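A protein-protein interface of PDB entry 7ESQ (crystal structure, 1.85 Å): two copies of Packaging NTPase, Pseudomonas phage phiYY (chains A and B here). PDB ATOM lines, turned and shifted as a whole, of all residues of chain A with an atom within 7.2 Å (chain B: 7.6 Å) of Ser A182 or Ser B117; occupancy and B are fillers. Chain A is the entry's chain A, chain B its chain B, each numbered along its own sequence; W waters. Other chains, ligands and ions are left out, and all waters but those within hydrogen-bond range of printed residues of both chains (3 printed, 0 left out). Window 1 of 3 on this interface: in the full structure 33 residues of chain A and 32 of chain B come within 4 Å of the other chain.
The backbone NH (N) of Leu A184 sits at hydrogen-bond distance from the backbone carbonyl oxygen (O) of Pro B114 (3.0 Å). The backbone carbonyl oxygen (O) of Ser A182 sits at hydrogen-bond distance from the backbone NH (N) of Ser B117 (2.7 Å). The side-chain amide nitrogen (ND2) of Asn A208 lies within hydrogen-bond range of the backbone carbonyl oxygen (O) of Leu B115, at 3.1 Å. ND2 of Asn B235 is in hydrogen-bond range of O of Glu A167 (2.8 Å). The backbone carbonyl oxygen (O) of Leu B116 sits at hydrogen-bond distance from the side-chain amide nitrogen (ND2) of Asn A208 (3.4 Å).
Of the printed residues of chain B, Ala A180 touches Arg B119 (3.6 Å) and Pro B120 (3.5 Å). Ser A182 touches just these residues of chain B: Leu B116 (3.5 Å), Ser B117 (2.7 Å) and Arg B119 (3.5 Å). Ala A187 touches none of the printed residues of chain B. Of the printed residues of chain A, Leu B115 touches Trp A165 and Asn A208. Of the printed residues of chain A, Thr B231 touches Gly A166, Glu A167 and Pro A168. The nearest residue of chain B that does not touch Ser A182 is Leu B115 (4.2 Å). The nearest printed residue of chain A that does not touch Ser B117 is Glu A167 (4.9 Å).
No position is printed for both chains.
Water W2 lies within hydrogen-bond range of the backbone carbonyl oxygen (O) of Leu B116 (2.8 Å) and the side-chain amide nitrogen (ND2) of Asn A208 (3.1 Å). Water W3 lies within hydrogen-bond range of O of Val A181, N of Gly A166, O of Val B118 and OG of Ser B117. Water W1 lies within hydrogen-bond range of NH2 of Arg B239, N of Arg B119 and OG of Ser A182.
Pro B120 touches Arg A164 (CG to CB, 3.8 Å). Thr B231 touches Gly A166. Glu A167 touches Thr B231 (C to CG2, 3.6 Å). O of Ala A180 touches CG of Arg B119, 3.6 Å away. Ala A180 touches Pro B120. C of Val A181 touches CG of Arg B119, at 3.5 Å. Arg B119 touches Ser A182 (CD to OG, 3.5 Å). Asp A183 touches Tyr B113. Pro B114 touches Asp A183 (O to CB, 3.3 Å). Ser B117 touches Asn A208 (CB to ND2, 3.7 Å).
Printed residues of chain B that touch a printed residue of chain A: Tyr B113, Pro B114, Leu B115, Leu B116, Ser B117, Arg B119, Pro B120, Ser B228, Thr B231 and Asn B235. Hydrophobic or aromatic side chains of chain B that line the printed part of chain A: Tyr B113, Pro B114, Leu B115, Leu B116 and Pro B120. Hydrophobic or aromatic side chains of chain A that line the printed part of chain B: Trp A165, Ala A180 and Leu A184. Among the printed residues, no Asp or Glu carboxylate lies within 4 Å of a Lys or Arg side-chain nitrogen of the other chain.
The side-chain carboxylate (OD1) of Asp A183 lies within hydrogen-bond range of the backbone NH (N) of Glu A186 (2.9 Å). The backbone carbonyl oxygen of Ser A182 sits at hydrogen-bond distance from the indole nitrogen of Trp A165 (3.2 Å). O of Arg A164 lies within hydrogen-bond range of N of Val A181 (3.0 Å). The side-chain amide nitrogen (ND2) of Asn B235 sits at hydrogen-bond distance from the backbone carbonyl oxygen (O) of Val B118 (3.0 Å). OD1 of Asp A183 lies within hydrogen-bond range of N of Asn A185 (3.0 Å). NH2 of Arg A164 sits at hydrogen-bond distance from O of Pro A168.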
ATOM      1  N   GLU A  94     -12.127 -21.018 -15.467  1.00  0.00           N
ATOM      2  CA  GLU A  94     -12.509 -20.830 -14.076  1.00  0.00           C
ATOM      3  C   GLU A  94     -12.646 -22.161 -13.353  1.00  0.00           C
ATOM      4  O   GLU A  94     -12.427 -22.227 -12.139  1.00  0.00           O
ATOM      5  CB  GLU A  94     -13.795 -20.010 -13.986  1.00  0.00           C
ATOM      6  CG  GLU A  94     -13.555 -18.554 -14.374  1.00  0.00           C
ATOM      7  CD  GLU A  94     -14.819 -17.722 -14.398  1.00  0.00           C
ATOM      8  OE1 GLU A  94     -14.707 -16.481 -14.282  1.00  0.00           O
ATOM      9  OE2 GLU A  94     -15.918 -18.305 -14.525  1.00  0.00           O
ATOM     10  N   HIS A  98     -10.611 -22.982  -9.859  1.00  0.00           N
ATOM     11  CA  HIS A  98     -11.238 -23.378  -8.602  1.00  0.00           C
ATOM     12  C   HIS A  98     -10.780 -24.755  -8.134  1.00  0.00           C
ATOM     13  O   HIS A  98     -11.000 -25.114  -6.968  1.00  0.00           O
ATOM     14  CB  HIS A  98     -12.752 -23.309  -8.745  1.00  0.00           C
ATOM     15  CG  HIS A  98     -13.283 -21.929  -8.534  1.00  0.00           C
ATOM     16  ND1 HIS A  98     -13.570 -21.083  -9.581  1.00  0.00           N
ATOM     17  CD2 HIS A  98     -13.519 -21.224  -7.401  1.00  0.00           C
ATOM     18  CE1 HIS A  98     -13.983 -19.922  -9.103  1.00  0.00           C
ATOM     19  NE2 HIS A  98     -13.965 -19.982  -7.783  1.00  0.00           N
ATOM     20  N   ARG A 164      -7.283  -7.787  -9.813  1.00  0.00           N
ATOM     21  CA  ARG A 164      -8.098  -6.815  -9.092  1.00  0.00           C
ATOM     22  C   ARG A 164      -9.131  -7.544  -8.234  1.00  0.00           C
ATOM     23  O   ARG A 164      -9.931  -8.329  -8.748  1.00  0.00           O
ATOM     24  CB  ARG A 164      -8.767  -5.853 -10.074  1.00  0.00           C
ATOM     25  CG  ARG A 164      -7.731  -4.952 -10.771  1.00  0.00           C
ATOM     26  CD  ARG A 164      -7.413  -3.734  -9.899  1.00  0.00           C
ATOM     27  NE  ARG A 164      -8.571  -2.830  -9.869  1.00  0.00           N
ATOM     28  CZ  ARG A 164      -8.743  -1.864  -8.974  1.00  0.00           C
ATOM     29  NH1 ARG A 164      -7.842  -1.656  -8.032  1.00  0.00           N
ATOM     30  NH2 ARG A 164      -9.826  -1.098  -9.017  1.00  0.00           N
ATOM     31  N   TRP A 165      -9.117  -7.272  -6.930  1.00  0.00           N
ATOM     32  CA  TRP A 165      -9.996  -7.990  -6.007  1.00  0.00           C
ATOM     33  C   TRP A 165     -10.379  -7.077  -4.854  1.00  0.00           C
ATOM     34  O   TRP A 165      -9.505  -6.472  -4.228  1.00  0.00           O
ATOM     35  CB  TRP A 165      -9.302  -9.254  -5.459  1.00  0.00           C
ATOM     36  CG  TRP A 165     -10.102  -9.972  -4.410  1.00  0.00           C
ATOM     37  CD1 TRP A 165     -11.431 -10.301  -4.475  1.00  0.00           C
ATOM     38  CD2 TRP A 165      -9.632 -10.454  -3.140  1.00  0.00           C
ATOM     39  NE1 TRP A 165     -11.819 -10.944  -3.310  1.00  0.00           N
ATOM     40  CE2 TRP A 165     -10.730 -11.056  -2.486  1.00  0.00           C
ATOM     41  CE3 TRP A 165      -8.390 -10.431  -2.496  1.00  0.00           C
ATOM     42  CZ2 TRP A 165     -10.623 -11.623  -1.224  1.00  0.00           C
ATOM     43  CZ3 TRP A 165      -8.281 -11.002  -1.232  1.00  0.00           C
ATOM     44  CH2 TRP A 165      -9.398 -11.584  -0.609  1.00  0.00           C
ATOM     45  N   GLY A 166     -11.673  -6.983  -4.572  1.00  0.00           N
ATOM     46  CA  GLY A 166     -12.105  -6.272  -3.388  1.00  0.00           C
ATOM     47  C   GLY A 166     -12.016  -4.769  -3.492  1.00  0.00           C
ATOM     48  O   GLY A 166     -12.150  -4.081  -2.471  1.00  0.00           O
ATOM     49  N   GLU A 167     -11.784  -4.244  -4.688  1.00  0.00           N
ATOM     50  CA  GLU A 167     -11.659  -2.812  -4.892  1.00  0.00           C
ATOM     51  C   GLU A 167     -12.759  -2.333  -5.834  1.00  0.00           C
ATOM     52  O   GLU A 167     -13.190  -3.091  -6.709  1.00  0.00           O
ATOM     53  CB  GLU A 167     -10.293  -2.464  -5.501  1.00  0.00           C
ATOM     54  CG  GLU A 167      -9.080  -2.727  -4.567  1.00  0.00           C
ATOM     55  CD  GLU A 167      -8.971  -1.728  -3.416  1.00  0.00           C
ATOM     56  OE1 GLU A 167      -8.470  -2.116  -2.335  1.00  0.00           O
ATOM     57  OE2 GLU A 167      -9.469  -0.587  -3.536  1.00  0.00           O
ATOM     58  N   PRO A 168     -13.205  -1.076  -5.719  1.00  0.00           N
ATOM     59  CA  PRO A 168     -14.239  -0.575  -6.639  1.00  0.00           C
ATOM     60  C   PRO A 168     -13.712  -0.444  -8.055  1.00  0.00           C
ATOM     61  O   PRO A 168     -12.520  -0.235  -8.276  1.00  0.00           O
ATOM     62  CB  PRO A 168     -14.588   0.805  -6.063  1.00  0.00           C
ATOM     63  CG  PRO A 168     -13.269   1.260  -5.426  1.00  0.00           C
ATOM     64  CD  PRO A 168     -12.697  -0.018  -4.821  1.00  0.00           C
ATOM     65  N   ALA A 180      -9.938  -9.340 -13.178  1.00  0.00           N
ATOM     66  CA  ALA A 180     -10.727  -9.142 -11.971  1.00  0.00           C
ATOM     67  C   ALA A 180     -11.212 -10.489 -11.437  1.00  0.00           C
ATOM     68  O   ALA A 180     -11.613 -11.361 -12.208  1.00  0.00           O
ATOM     69  CB  ALA A 180     -11.914  -8.219 -12.264  1.00  0.00           C
ATOM     70  N   VAL A 181     -11.184 -10.647 -10.114  1.00  0.00           N
ATOM     71  CA  VAL A 181     -11.670 -11.857  -9.445  1.00  0.00           C
ATOM     72  C   VAL A 181     -12.630 -11.471  -8.312  1.00  0.00           C
ATOM     73  O   VAL A 181     -12.817 -10.293  -7.999  1.00  0.00           O
ATOM     74  CB  VAL A 181     -10.512 -12.736  -8.916  1.00  0.00           C
ATOM     75  CG1 VAL A 181      -9.566 -13.139 -10.072  1.00  0.00           C
ATOM     76  CG2 VAL A 181      -9.743 -12.002  -7.824  1.00  0.00           C
ATOM     77  N   SER A 182     -13.243 -12.497  -7.688  1.00  0.00           N
ATOM     78  CA  SER A 182     -14.296 -12.333  -6.685  1.00  0.00           C
ATOM     79  C   SER A 182     -13.938 -12.820  -5.284  1.00  0.00           C
ATOM     80  O   SER A 182     -14.545 -12.347  -4.315  1.00  0.00           O
ATOM     81  CB  SER A 182     -15.564 -13.103  -7.108  1.00  0.00           C
ATOM     82  OG  SER A 182     -15.941 -12.805  -8.416  1.00  0.00           O
ATOM     83  N   ASP A 183     -13.025 -13.785  -5.127  1.00  0.00           N
ATOM     84  CA  ASP A 183     -12.776 -14.324  -3.784  1.00  0.00           C
ATOM     85  C   ASP A 183     -11.303 -14.685  -3.631  1.00  0.00           C
ATOM     86  O   ASP A 183     -10.515 -14.613  -4.586  1.00  0.00           O
ATOM     87  CB  ASP A 183     -13.702 -15.528  -3.462  1.00  0.00           C
ATOM     88  CG  ASP A 183     -13.394 -16.791  -4.304  1.00  0.00           C
ATOM     89  OD1 ASP A 183     -12.214 -17.170  -4.473  1.00  0.00           O
ATOM     90  OD2 ASP A 183     -14.349 -17.452  -4.765  1.00  0.00           O
ATOM     91  N   LEU A 184     -10.929 -15.051  -2.401  1.00  0.00           N
ATOM     92  CA  LEU A 184      -9.513 -15.232  -2.093  1.00  0.00           C
ATOM     93  C   LEU A 184      -8.934 -16.459  -2.792  1.00  0.00           C
ATOM     94  O   LEU A 184      -7.775 -16.419  -3.228  1.00  0.00           O
ATOM     95  CB  LEU A 184      -9.289 -15.300  -0.584  1.00  0.00           C
ATOM     96  CG  LEU A 184      -7.825 -15.500  -0.141  1.00  0.00           C
ATOM     97  CD1 LEU A 184      -6.894 -14.361  -0.648  1.00  0.00           C
ATOM     98  CD2 LEU A 184      -7.734 -15.628   1.363  1.00  0.00           C
ATOM     99  N   ASN A 185      -9.698 -17.562  -2.910  1.00  0.00           N
ATOM    100  CA  ASN A 185      -9.226 -18.675  -3.754  1.00  0.00           C
ATOM    101  C   ASN A 185      -8.810 -18.217  -5.140  1.00  0.00           C
ATOM    102  O   ASN A 185      -7.723 -18.573  -5.618  1.00  0.00           O
ATOM    103  CB  ASN A 185     -10.249 -19.825  -3.889  1.00  0.00           C
ATOM    104  CG  ASN A 185     -10.618 -20.463  -2.570  1.00  0.00           C
ATOM    105  OD1 ASN A 185      -9.781 -20.538  -1.665  1.00  0.00           O
ATOM    106  ND2 ASN A 185     -11.845 -20.970  -2.461  1.00  0.00           N
ATOM    107  N   GLU A 186      -9.688 -17.479  -5.820  1.00  0.00           N
ATOM    108  CA  GLU A 186      -9.404 -17.035  -7.182  1.00  0.00           C
ATOM    109  C   GLU A 186      -8.179 -16.141  -7.242  1.00  0.00           C
ATOM    110  O   GLU A 186      -7.341 -16.288  -8.144  1.00  0.00           O
ATOM    111  CB  GLU A 186     -10.628 -16.311  -7.723  1.00  0.00           C
ATOM    112  CG  GLU A 186     -11.820 -17.219  -7.952  1.00  0.00           C
ATOM    113  CD  GLU A 186     -13.046 -16.431  -8.415  1.00  0.00           C
ATOM    114  OE1 GLU A 186     -12.899 -15.231  -8.695  1.00  0.00           O
ATOM    115  OE2 GLU A 186     -14.121 -17.042  -8.625  1.00  0.00           O
ATOM    116  N   ALA A 187      -8.073 -15.185  -6.312  1.00  0.00           N
ATOM    117  CA  ALA A 187      -6.936 -14.269  -6.317  1.00  0.00           C
ATOM    118  C   ALA A 187      -5.625 -15.027  -6.142  1.00  0.00           C
ATOM    119  O   ALA A 187      -4.643 -14.781  -6.860  1.00  0.00           O
ATOM    120  CB  ALA A 187      -7.105 -13.222  -5.207  1.00  0.00           C
ATOM    121  N   ASN A 208     -10.059  -7.158   1.722  1.00  0.00           N
ATOM    122  CA  ASN A 208     -11.016  -7.970   2.461  1.00  0.00           C
ATOM    123  C   ASN A 208     -10.366  -8.838   3.526  1.00  0.00           C
ATOM    124  O   ASN A 208     -11.067  -9.298   4.435  1.00  0.00           O
ATOM    125  CB  ASN A 208     -11.841  -8.815   1.495  1.00  0.00           C
ATOM    126  CG  ASN A 208     -13.032  -8.047   0.952  1.00  0.00           C
ATOM    127  OD1 ASN A 208     -13.155  -6.829   1.170  1.00  0.00           O
ATOM    128  ND2 ASN A 208     -13.939  -8.750   0.280  1.00  0.00           N
ATOM    129  N   ILE B  57     -25.264 -13.532  -9.690  1.00  0.00           N
ATOM    130  CA  ILE B  57     -24.104 -12.829  -9.156  1.00  0.00           C
ATOM    131  C   ILE B  57     -24.288 -12.734  -7.650  1.00  0.00           C
ATOM    132  O   ILE B  57     -25.295 -12.191  -7.190  1.00  0.00           O
ATOM    133  CB  ILE B  57     -23.943 -11.428  -9.766  1.00  0.00           C
ATOM    134  CG1 ILE B  57     -23.746 -11.514 -11.279  1.00  0.00           C
ATOM    135  CG2 ILE B  57     -22.756 -10.705  -9.127  1.00  0.00           C
ATOM    136  CD1 ILE B  57     -23.675 -10.161 -11.924  1.00  0.00           C
ATOM    137  N   MET B  58     -23.342 -13.270  -6.875  1.00  0.00           N
ATOM    138  CA  MET B  58     -23.515 -13.123  -5.435  1.00  0.00           C
ATOM    139  C   MET B  58     -23.053 -11.758  -4.942  1.00  0.00           C
ATOM    140  O   MET B  58     -22.112 -11.159  -5.468  1.00  0.00           O
ATOM    141  CB  MET B  58     -22.838 -14.234  -4.611  1.00  0.00           C
ATOM    142  CG  MET B  58     -23.047 -15.648  -5.129  1.00  0.00           C
ATOM    143  SD  MET B  58     -21.999 -16.877  -4.280  1.00  0.00           S
ATOM    144  CE  MET B  58     -20.525 -16.726  -5.273  1.00  0.00           C
ATOM    145  N   ILE B  59     -23.739 -11.278  -3.910  1.00  0.00           N
ATOM    146  CA  ILE B  59     -23.514  -9.947  -3.338  1.00  0.00           C
ATOM    147  C   ILE B  59     -23.252 -10.115  -1.848  1.00  0.00           C
ATOM    148  O   ILE B  59     -24.199 -10.302  -1.075  1.00  0.00           O
ATOM    149  CB  ILE B  59     -24.718  -9.015  -3.573  1.00  0.00           C
ATOM    150  CG1 ILE B  59     -25.198  -9.101  -5.031  1.00  0.00           C
ATOM    151  CG2 ILE B  59     -24.348  -7.576  -3.194  1.00  0.00           C
ATOM    152  CD1 ILE B  59     -26.465  -8.186  -5.360  1.00  0.00           C
ATOM    153  N   PRO B  60     -22.001 -10.061  -1.397  1.00  0.00           N
ATOM    154  CA  PRO B  60     -21.738 -10.143   0.049  1.00  0.00           C
ATOM    155  C   PRO B  60     -22.004  -8.802   0.735  1.00  0.00           C
ATOM    156  O   PRO B  60     -21.525  -7.761   0.286  1.00  0.00           O
ATOM    157  CB  PRO B  60     -20.250 -10.514   0.117  1.00  0.00           C
ATOM    158  CG  PRO B  60     -19.659  -9.942  -1.171  1.00  0.00           C
ATOM    159  CD  PRO B  60     -20.779  -9.873  -2.199  1.00  0.00           C
ATOM    160  N   TYR B 113     -16.569 -19.655  -0.897  1.00  0.00           N
ATOM    161  CA  TYR B 113     -16.155 -18.418  -1.561  1.00  0.00           C
ATOM    162  C   TYR B 113     -15.533 -17.488  -0.524  1.00  0.00           C
ATOM    163  O   TYR B 113     -16.175 -16.525  -0.080  1.00  0.00           O
ATOM    164  CB  TYR B 113     -17.354 -17.762  -2.262  1.00  0.00           C
ATOM    165  CG  TYR B 113     -18.020 -18.734  -3.213  1.00  0.00           C
ATOM    166  CD1 TYR B 113     -17.439 -19.024  -4.441  1.00  0.00           C
ATOM    167  CD2 TYR B 113     -19.195 -19.406  -2.864  1.00  0.00           C
ATOM    168  CE1 TYR B 113     -18.006 -19.939  -5.307  1.00  0.00           C
ATOM    169  CE2 TYR B 113     -19.781 -20.332  -3.742  1.00  0.00           C
ATOM    170  CZ  TYR B 113     -19.171 -20.585  -4.953  1.00  0.00           C
ATOM    171  OH  TYR B 113     -19.703 -21.481  -5.846  1.00  0.00           O
ATOM    172  N   PRO B 114     -14.282 -17.734  -0.128  1.00  0.00           N
ATOM    173  CA  PRO B 114     -13.705 -17.012   1.024  1.00  0.00           C
ATOM    174  C   PRO B 114     -13.527 -15.519   0.755  1.00  0.00           C
ATOM    175  O   PRO B 114     -12.976 -15.123  -0.275  1.00  0.00           O
ATOM    176  CB  PRO B 114     -12.350 -17.699   1.238  1.00  0.00           C
ATOM    177  CG  PRO B 114     -12.024 -18.330  -0.087  1.00  0.00           C
ATOM    178  CD  PRO B 114     -13.350 -18.728  -0.699  1.00  0.00           C
ATOM    179  N   LEU B 115     -13.967 -14.700   1.717  1.00  0.00           N
ATOM    180  CA  LEU B 115     -13.794 -13.238   1.673  1.00  0.00           C
ATOM    181  C   LEU B 115     -14.371 -12.664   0.383  1.00  0.00           C
ATOM    182  O   LEU B 115     -13.802 -11.769  -0.244  1.00  0.00           O
ATOM    183  CB  LEU B 115     -12.324 -12.851   1.859  1.00  0.00           C
ATOM    184  CG  LEU B 115     -11.722 -13.369   3.181  1.00  0.00           C
ATOM    185  CD1 LEU B 115     -10.232 -13.077   3.226  1.00  0.00           C
ATOM    186  CD2 LEU B 115     -12.427 -12.752   4.417  1.00  0.00           C
ATOM    187  N   LEU B 116     -15.534 -13.182   0.001  1.00  0.00           N
ATOM    188  CA  LEU B 116     -16.168 -12.844  -1.263  1.00  0.00           C
ATOM    189  C   LEU B 116     -16.333 -11.333  -1.443  1.00  0.00           C
ATOM    190  O   LEU B 116     -16.649 -10.599  -0.501  1.00  0.00           O
ATOM    191  CB  LEU B 116     -17.527 -13.542  -1.329  1.00  0.00           C
ATOM    192  CG  LEU B 116     -18.414 -13.318  -2.549  1.00  0.00           C
ATOM    193  CD1 LEU B 116     -17.789 -13.986  -3.761  1.00  0.00           C
ATOM    194  CD2 LEU B 116     -19.783 -13.939  -2.264  1.00  0.00           C
ATOM    195  N   SER B 117     -16.097 -10.882  -2.669  1.00  0.00           N
ATOM    196  CA  SER B 117     -16.407  -9.520  -3.101  1.00  0.00           C
ATOM    197  C   SER B 117     -17.189  -9.660  -4.407  1.00  0.00           C
ATOM    198  O   SER B 117     -17.784 -10.710  -4.692  1.00  0.00           O
ATOM    199  CB  SER B 117     -15.108  -8.703  -3.236  1.00  0.00           C
ATOM    200  OG  SER B 117     -15.365  -7.355  -3.632  1.00  0.00           O
ATOM    201  N   VAL B 118     -17.173  -8.605  -5.228  1.00  0.00           N
ATOM    202  CA  VAL B 118     -17.768  -8.610  -6.563  1.00  0.00           C
ATOM    203  C   VAL B 118     -16.717  -8.081  -7.525  1.00  0.00           C
ATOM    204  O   VAL B 118     -16.029  -7.099  -7.215  1.00  0.00           O
ATOM    205  CB  VAL B 118     -19.049  -7.747  -6.653  1.00  0.00           C
ATOM    206  CG1 VAL B 118     -19.603  -7.747  -8.098  1.00  0.00           C
ATOM    207  CG2 VAL B 118     -20.112  -8.234  -5.688  1.00  0.00           C
ATOM    208  N   ARG B 119     -16.590  -8.738  -8.669  1.00  0.00           N
ATOM    209  CA  ARG B 119     -15.556  -8.419  -9.651  1.00  0.00           C
ATOM    210  C   ARG B 119     -15.712  -6.974 -10.120  1.00  0.00           C
ATOM    211  O   ARG B 119     -16.807  -6.596 -10.550  1.00  0.00           O
ATOM    212  CB  ARG B 119     -15.726  -9.362 -10.842  1.00  0.00           C
ATOM    213  CG  ARG B 119     -14.818 -10.549 -10.867  1.00  0.00           C
ATOM    214  CD  ARG B 119     -15.459 -11.675 -11.680  1.00  0.00           C
ATOM    215  NE  ARG B 119     -15.823 -11.285 -13.042  1.00  0.00           N
ATOM    216  CZ  ARG B 119     -16.620 -12.009 -13.830  1.00  0.00           C
ATOM    217  NH1 ARG B 119     -17.141 -13.148 -13.387  1.00  0.00           N
ATOM    218  NH2 ARG B 119     -16.912 -11.593 -15.054  1.00  0.00           N
ATOM    219  N   PRO B 120     -14.638  -6.137 -10.078  1.00  0.00           N
ATOM    220  CA  PRO B 120     -14.718  -4.788 -10.671  1.00  0.00           C
ATOM    221  C   PRO B 120     -14.642  -4.875 -12.190  1.00  0.00           C
ATOM    222  O   PRO B 120     -13.593  -5.199 -12.756  1.00  0.00           O
ATOM    223  CB  PRO B 120     -13.489  -4.072 -10.083  1.00  0.00           C
ATOM    224  CG  PRO B 120     -12.539  -5.175  -9.721  1.00  0.00           C
ATOM    225  CD  PRO B 120     -13.429  -6.315  -9.264  1.00  0.00           C
ATOM    226  N   SER B 228     -16.613  -2.376   2.635  1.00  0.00           N
ATOM    227  CA  SER B 228     -16.618  -3.504   1.700  1.00  0.00           C
ATOM    228  C   SER B 228     -18.022  -3.788   1.172  1.00  0.00           C
ATOM    229  O   SER B 228     -18.182  -4.211   0.017  1.00  0.00           O
ATOM    230  CB  SER B 228     -16.028  -4.754   2.367  1.00  0.00           C
ATOM    231  OG  SER B 228     -16.793  -5.151   3.496  1.00  0.00           O
ATOM    232  N   THR B 231     -18.509  -1.294  -1.564  1.00  0.00           N
ATOM    233  CA  THR B 231     -17.744  -1.695  -2.749  1.00  0.00           C
ATOM    234  C   THR B 231     -18.407  -2.870  -3.476  1.00  0.00           C
ATOM    235  O   THR B 231     -18.479  -2.884  -4.714  1.00  0.00           O
ATOM    236  CB  THR B 231     -16.302  -2.038  -2.353  1.00  0.00           C
ATOM    237  OG1 THR B 231     -15.619  -0.849  -1.916  1.00  0.00           O
ATOM    238  CG2 THR B 231     -15.532  -2.644  -3.528  1.00  0.00           C
ATOM    239  N   ALA B 232     -18.881  -3.870  -2.728  1.00  0.00           N
ATOM    240  CA  ALA B 232     -19.575  -5.005  -3.342  1.00  0.00           C
ATOM    241  C   ALA B 232     -20.792  -4.547  -4.147  1.00  0.00           C
ATOM    242  O   ALA B 232     -20.937  -4.889  -5.326  1.00  0.00           O
ATOM    243  CB  ALA B 232     -19.996  -5.998  -2.258  1.00  0.00           C
ATOM    244  N   ILE B 233     -21.681  -3.767  -3.525  1.00  0.00           N
ATOM    245  CA  ILE B 233     -22.856  -3.270  -4.243  1.00  0.00           C
ATOM    246  C   ILE B 233     -22.448  -2.349  -5.386  1.00  0.00           C
ATOM    247  O   ILE B 233     -23.023  -2.412  -6.481  1.00  0.00           O
ATOM    248  CB  ILE B 233     -23.827  -2.588  -3.262  1.00  0.00           C
ATOM    249  CG1 ILE B 233     -24.340  -3.624  -2.249  1.00  0.00           C
ATOM    250  CG2 ILE B 233     -24.982  -1.915  -4.003  1.00  0.00           C
ATOM    251  CD1 ILE B 233     -25.027  -3.011  -1.026  1.00  0.00           C
ATOM    252  N   ASN B 235     -19.796  -2.598  -7.180  1.00  0.00           N
ATOM    253  CA  ASN B 235     -19.313  -3.384  -8.312  1.00  0.00           C
ATOM    254  C   ASN B 235     -20.416  -4.209  -8.973  1.00  0.00           C
ATOM    255  O   ASN B 235     -20.288  -4.547 -10.164  1.00  0.00           O
ATOM    256  CB  ASN B 235     -18.124  -4.262  -7.892  1.00  0.00           C
ATOM    257  CG  ASN B 235     -16.861  -3.439  -7.616  1.00  0.00           C
ATOM    258  OD1 ASN B 235     -16.829  -2.228  -7.894  1.00  0.00           O
ATOM    259  ND2 ASN B 235     -15.800  -4.091  -7.115  1.00  0.00           N
ATOM    260  N   VAL B 236     -21.526  -4.506  -8.284  1.00  0.00           N
ATOM    261  CA  VAL B 236     -22.666  -5.036  -9.035  1.00  0.00           C
ATOM    262  C   VAL B 236     -23.138  -3.993 -10.034  1.00  0.00           C
ATOM    263  O   VAL B 236     -23.385  -4.288 -11.211  1.00  0.00           O
ATOM    264  CB  VAL B 236     -23.820  -5.457  -8.104  1.00  0.00           C
ATOM    265  CG1 VAL B 236     -24.999  -5.963  -8.961  1.00  0.00           C
ATOM    266  CG2 VAL B 236     -23.373  -6.529  -7.131  1.00  0.00           C
ATOM    267  N   ARG B 239     -20.688  -3.860 -12.971  1.00  0.00           N
ATOM    268  CA  ARG B 239     -20.885  -4.960 -13.916  1.00  0.00           C
ATOM    269  C   ARG B 239     -22.154  -4.766 -14.743  1.00  0.00           C
ATOM    270  O   ARG B 239     -22.214  -5.185 -15.908  1.00  0.00           O
ATOM    271  CB  ARG B 239     -20.925  -6.299 -13.168  1.00  0.00           C
ATOM    272  CG  ARG B 239     -19.567  -6.718 -12.561  1.00  0.00           C
ATOM    273  CD  ARG B 239     -19.580  -8.133 -11.971  1.00  0.00           C
ATOM    274  NE  ARG B 239     -19.955  -9.159 -12.951  1.00  0.00           N
ATOM    275  CZ  ARG B 239     -20.045 -10.462 -12.681  1.00  0.00           C
ATOM    276  NH1 ARG B 239     -20.405 -11.310 -13.631  1.00  0.00           N
ATOM    277  NH2 ARG B 239     -19.801 -10.922 -11.457  1.00  0.00           N
HETATM  278  O   HOH W   1     -18.402 -11.060  -9.002  1.00  0.00           O
HETATM  279  O   HOH W   2     -16.909  -7.907   0.123  1.00  0.00           O
HETATM  280  O   HOH W   3     -13.541  -8.258  -6.254  1.00  0.00           O
